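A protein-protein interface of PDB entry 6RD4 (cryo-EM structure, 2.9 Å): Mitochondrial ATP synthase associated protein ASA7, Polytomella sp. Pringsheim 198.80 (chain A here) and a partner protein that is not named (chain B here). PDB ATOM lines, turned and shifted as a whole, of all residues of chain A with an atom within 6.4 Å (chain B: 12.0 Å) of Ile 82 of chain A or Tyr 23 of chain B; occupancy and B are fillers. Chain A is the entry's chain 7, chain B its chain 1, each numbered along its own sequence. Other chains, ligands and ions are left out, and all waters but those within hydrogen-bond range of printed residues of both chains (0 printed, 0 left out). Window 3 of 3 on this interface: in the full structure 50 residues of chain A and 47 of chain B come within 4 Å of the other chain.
The side-chain hydroxyl (OG) of Ser 155 of chain A lies close to the backbone carbonyl oxygen (O) of Tyr 23 of chain B.
A ring nitrogen (NE2) of His 86 of chain A lies close to the backbone carbonyl oxygen of Ser 151 of chain A (3.1 Å). The guanidinium group of Arg 81 of chain A sits at hydrogen-bond distance from the side-chain hydroxyl of Ser 151 of chain A. The side-chain hydroxyl (OG) of Ser 83 of chain A sits at hydrogen-bond distance from the backbone NH (N) of His 86 of chain A, at 3.3 Å. The side-chain hydroxyl of Ser 155 of chain A lies close to a ring nitrogen (ND1) of His 86 of chain A (3.5 Å).
NH1 of Arg 81 of chain A touches CD1 of Tyr 23 of chain B, 3.6 Å away. Tyr 23 of chain B touches Ile 82 of chain A. His 86 of chain A touches Tyr 23 of chain B. OG of Ser 151 of chain A touches CB of Tyr 23 of chain B (3.5 Å). Ala 152 of chain A touches Tyr 23 of chain B. Ser 155 of chain A touches Leu 24 of chain B. Ser 155 of chain A touches Ala 25 of chain B (O to CB, 3.8 Å).
Ala 80 of chain A touches none of the printed residues of chain B. Of the printed residues of chain B, Arg 81 of chain A touches Tyr 23 (3.6 Å). No residue of chain B comes within 4 Å of Ser 83 of chain A. Of the printed residues of chain B, His 86 of chain A touches Tyr 23 (3.8 Å). Ser 151 of chain A touches just one residue of chain B: Tyr 23 (3.5 Å). Printed residues of chain B within 4 Å of Ala 152 of chain A: Tyr 23 (3.9 Å). No residue of chain B comes within 4 Å of Ala 154 of chain A. Of chain B, only Tyr 23, Leu 24 and Ala 25 come within 4 Å of Ser 155 of chain A. Of the printed residues of chain A, Leu 24 of chain B touches Ser 155 (3.98 Å). Printed residues of chain A within 4 Å of Ala 25 of chain B: Ser 155 (3.8 Å). The nearest residue of chain B that does not touch Ile 82 of chain A is Leu 24 of chain B (5.3 Å). The nearest printed residue of chain A that does not touch Leu 24 of chain B is Ile 82 of chain A (5.3 Å).
Of the 5 printed residues of chain B, 3 touch a printed residue of chain A. Printed residues of chain B that touch a printed residue of chain A: Tyr 23, Leu 24 and Ala 25. Hydrophobic or aromatic side chains of chain A that line the printed part of chain B: Ile 82, His 86 and Ala 152.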
ATOM      1  N   ALA A  80      -5.371 -28.622   4.214  1.00  0.00           N
ATOM      2  CA  ALA A  80      -5.425 -27.692   5.321  1.00  0.00           C
ATOM      3  C   ALA A  80      -6.572 -26.728   5.116  1.00  0.00           C
ATOM      4  O   ALA A  80      -7.056 -26.544   4.003  1.00  0.00           O
ATOM      5  CB  ALA A  80      -4.114 -26.937   5.449  1.00  0.00           C
ATOM      6  N   ARG A  81      -7.029 -26.137   6.214  1.00  0.00           N
ATOM      7  CA  ARG A  81      -8.122 -25.186   6.111  1.00  0.00           C
ATOM      8  C   ARG A  81      -7.664 -23.929   5.414  1.00  0.00           C
ATOM      9  O   ARG A  81      -8.318 -23.446   4.490  1.00  0.00           O
ATOM     10  CB  ARG A  81      -8.676 -24.849   7.483  1.00  0.00           C
ATOM     11  CG  ARG A  81      -9.694 -23.769   7.427  1.00  0.00           C
ATOM     12  CD  ARG A  81     -10.491 -23.717   8.662  1.00  0.00           C
ATOM     13  NE  ARG A  81     -11.421 -22.604   8.642  1.00  0.00           N
ATOM     14  CZ  ARG A  81     -11.186 -21.450   9.238  1.00  0.00           C
ATOM     15  NH1 ARG A  81     -12.078 -20.483   9.191  1.00  0.00           N
ATOM     16  NH2 ARG A  81     -10.052 -21.268   9.882  1.00  0.00           N
ATOM     17  N   ILE A  82      -6.524 -23.400   5.825  1.00  0.00           N
ATOM     18  CA  ILE A  82      -5.916 -22.249   5.187  1.00  0.00           C
ATOM     19  C   ILE A  82      -4.593 -22.622   4.540  1.00  0.00           C
ATOM     20  O   ILE A  82      -4.465 -22.582   3.322  1.00  0.00           O
ATOM     21  CB  ILE A  82      -5.760 -21.087   6.183  1.00  0.00           C
ATOM     22  CG1 ILE A  82      -7.143 -20.617   6.588  1.00  0.00           C
ATOM     23  CG2 ILE A  82      -5.011 -19.972   5.559  1.00  0.00           C
ATOM     24  CD1 ILE A  82      -7.146 -19.547   7.576  1.00  0.00           C
ATOM     25  N   SER A  83      -3.623 -23.052   5.330  1.00  0.00           N
ATOM     26  CA  SER A  83      -2.369 -23.539   4.787  1.00  0.00           C
ATOM     27  C   SER A  83      -1.730 -24.421   5.836  1.00  0.00           C
ATOM     28  O   SER A  83      -2.221 -24.528   6.953  1.00  0.00           O
ATOM     29  CB  SER A  83      -1.447 -22.395   4.379  1.00  0.00           C
ATOM     30  OG  SER A  83      -1.230 -21.497   5.435  1.00  0.00           O
ATOM     31  N   VAL A  84      -0.659 -25.097   5.448  1.00  0.00           N
ATOM     32  CA  VAL A  84       0.071 -25.925   6.393  1.00  0.00           C
ATOM     33  C   VAL A  84       0.871 -25.065   7.345  1.00  0.00           C
ATOM     34  O   VAL A  84       1.083 -25.442   8.498  1.00  0.00           O
ATOM     35  CB  VAL A  84       0.957 -26.906   5.624  1.00  0.00           C
ATOM     36  CG1 VAL A  84       1.542 -27.899   6.523  1.00  0.00           C
ATOM     37  CG2 VAL A  84       0.132 -27.619   4.640  1.00  0.00           C
ATOM     38  N   HIS A  86      -0.066 -21.974   8.451  1.00  0.00           N
ATOM     39  CA  HIS A  86      -1.027 -21.386   9.362  1.00  0.00           C
ATOM     40  C   HIS A  86      -1.543 -22.395  10.359  1.00  0.00           C
ATOM     41  O   HIS A  86      -1.722 -22.070  11.527  1.00  0.00           O
ATOM     42  CB  HIS A  86      -2.162 -20.820   8.542  1.00  0.00           C
ATOM     43  CG  HIS A  86      -3.240 -20.187   9.342  1.00  0.00           C
ATOM     44  ND1 HIS A  86      -3.347 -18.827   9.483  1.00  0.00           N
ATOM     45  CD2 HIS A  86      -4.295 -20.717   9.996  1.00  0.00           C
ATOM     46  CE1 HIS A  86      -4.402 -18.551  10.217  1.00  0.00           C
ATOM     47  NE2 HIS A  86      -4.997 -19.680  10.538  1.00  0.00           N
ATOM     48  N   SER A  87      -1.759 -23.624   9.927  1.00  0.00           N
ATOM     49  CA  SER A  87      -2.245 -24.666  10.807  1.00  0.00           C
ATOM     50  C   SER A  87      -1.211 -25.107  11.809  1.00  0.00           C
ATOM     51  O   SER A  87      -1.566 -25.718  12.805  1.00  0.00           O
ATOM     52  CB  SER A  87      -2.681 -25.854   9.983  1.00  0.00           C
ATOM     53  OG  SER A  87      -3.821 -25.506   9.239  1.00  0.00           O
ATOM     54  N   SER A 151      -7.553 -18.948  15.382  1.00  0.00           N
ATOM     55  CA  SER A 151      -7.264 -19.006  13.964  1.00  0.00           C
ATOM     56  C   SER A 151      -7.032 -17.648  13.358  1.00  0.00           C
ATOM     57  O   SER A 151      -6.495 -17.573  12.262  1.00  0.00           O
ATOM     58  CB  SER A 151      -8.394 -19.677  13.212  1.00  0.00           C
ATOM     59  OG  SER A 151      -8.256 -19.431  11.834  1.00  0.00           O
ATOM     60  N   ALA A 152      -7.437 -16.581  14.018  1.00  0.00           N
ATOM     61  CA  ALA A 152      -7.138 -15.245  13.547  1.00  0.00           C
ATOM     62  C   ALA A 152      -5.951 -14.641  14.251  1.00  0.00           C
ATOM     63  O   ALA A 152      -5.455 -13.611  13.807  1.00  0.00           O
ATOM     64  CB  ALA A 152      -8.342 -14.330  13.730  1.00  0.00           C
ATOM     65  N   LEU A 153      -5.513 -15.240  15.351  1.00  0.00           N
ATOM     66  CA  LEU A 153      -4.240 -14.863  15.938  1.00  0.00           C
ATOM     67  C   LEU A 153      -3.089 -15.481  15.189  1.00  0.00           C
ATOM     68  O   LEU A 153      -1.965 -14.992  15.275  1.00  0.00           O
ATOM     69  CB  LEU A 153      -4.150 -15.312  17.381  1.00  0.00           C
ATOM     70  CG  LEU A 153      -5.017 -14.764  18.473  1.00  0.00           C
ATOM     71  CD1 LEU A 153      -4.530 -15.413  19.695  1.00  0.00           C
ATOM     72  CD2 LEU A 153      -4.804 -13.309  18.536  1.00  0.00           C
ATOM     73  N   ALA A 154      -3.329 -16.588  14.499  1.00  0.00           N
ATOM     74  CA  ALA A 154      -2.287 -17.184  13.698  1.00  0.00           C
ATOM     75  C   ALA A 154      -2.017 -16.378  12.448  1.00  0.00           C
ATOM     76  O   ALA A 154      -0.920 -16.458  11.909  1.00  0.00           O
ATOM     77  CB  ALA A 154      -2.669 -18.604  13.339  1.00  0.00           C
ATOM     78  N   SER A 155      -2.976 -15.598  11.982  1.00  0.00           N
ATOM     79  CA  SER A 155      -2.782 -14.719  10.844  1.00  0.00           C
ATOM     80  C   SER A 155      -2.116 -13.413  11.203  1.00  0.00           C
ATOM     81  O   SER A 155      -1.927 -12.573  10.327  1.00  0.00           O
ATOM     82  CB  SER A 155      -4.110 -14.415  10.194  1.00  0.00           C
ATOM     83  OG  SER A 155      -4.640 -15.581   9.638  1.00  0.00           O
ATOM     84  N   TYR B  23      -9.557 -14.686  10.017  1.00  0.00           N
ATOM     85  CA  TYR B  23      -8.555 -15.712   9.817  1.00  0.00           C
ATOM     86  C   TYR B  23      -7.620 -15.317   8.709  1.00  0.00           C
ATOM     87  O   TYR B  23      -6.581 -15.923   8.519  1.00  0.00           O
ATOM     88  CB  TYR B  23      -9.201 -17.052   9.496  1.00  0.00           C
ATOM     89  CG  TYR B  23     -10.235 -17.019   8.403  1.00  0.00           C
ATOM     90  CD1 TYR B  23     -11.574 -16.919   8.709  1.00  0.00           C
ATOM     91  CD2 TYR B  23      -9.875 -17.115   7.071  1.00  0.00           C
ATOM     92  CE1 TYR B  23     -12.515 -16.898   7.731  1.00  0.00           C
ATOM     93  CE2 TYR B  23     -10.811 -17.090   6.089  1.00  0.00           C
ATOM     94  CZ  TYR B  23     -12.130 -16.981   6.427  1.00  0.00           C
ATOM     95  OH  TYR B  23     -13.084 -16.960   5.450  1.00  0.00           O
ATOM     96  N   LEU B  24      -8.012 -14.314   7.949  1.00  0.00           N
ATOM     97  CA  LEU B  24      -7.257 -13.904   6.781  1.00  0.00           C
ATOM     98  C   LEU B  24      -6.313 -12.753   7.091  1.00  0.00           C
ATOM     99  O   LEU B  24      -6.548 -11.948   7.992  1.00  0.00           O
ATOM    100  CB  LEU B  24      -8.207 -13.563   5.635  1.00  0.00           C
ATOM    101  CG  LEU B  24      -9.565 -12.960   5.944  1.00  0.00           C
ATOM    102  CD1 LEU B  24      -9.456 -11.560   6.317  1.00  0.00           C
ATOM    103  CD2 LEU B  24     -10.383 -13.066   4.704  1.00  0.00           C
ATOM    104  N   ALA B  25      -5.237 -12.696   6.331  1.00  0.00           N
ATOM    105  CA  ALA B  25      -4.093 -11.855   6.597  1.00  0.00           C
ATOM    106  C   ALA B  25      -3.975 -10.753   5.558  1.00  0.00           C
ATOM    107  O   ALA B  25      -4.518 -10.868   4.454  1.00  0.00           O
ATOM    108  CB  ALA B  25      -2.819 -12.709   6.595  1.00  0.00           C
ATOM    109  N   PRO B  26      -3.296  -9.654   5.877  1.00  0.00           N
ATOM    110  CA  PRO B  26      -2.948  -8.687   4.834  1.00  0.00           C
ATOM    111  C   PRO B  26      -1.886  -9.254   3.910  1.00  0.00           C
ATOM    112  O   PRO B  26      -0.886  -9.815   4.360  1.00  0.00           O
ATOM    113  CB  PRO B  26      -2.425  -7.486   5.622  1.00  0.00           C
ATOM    114  CG  PRO B  26      -2.039  -8.033   6.921  1.00  0.00           C
ATOM    115  CD  PRO B  26      -2.991  -9.129   7.213  1.00  0.00           C
ATOM    116  N   LEU B  27      -2.111  -9.115   2.613  1.00  0.00           N
ATOM    117  CA  LEU B  27      -1.150  -9.585   1.635  1.00  0.00           C
ATOM    118  C   LEU B  27      -0.024  -8.574   1.488  1.00  0.00           C
ATOM    119  O   LEU B  27      -0.270  -7.374   1.361  1.00  0.00           O
ATOM    120  CB  LEU B  27      -1.830  -9.819   0.292  1.00  0.00           C
ATOM    121  CG  LEU B  27      -2.785 -10.992   0.157  1.00  0.00           C
ATOM    122  CD1 LEU B  27      -3.100 -11.224  -1.291  1.00  0.00           C
ATOM    123  CD2 LEU B  27      -2.202 -12.229   0.768  1.00  0.00           C
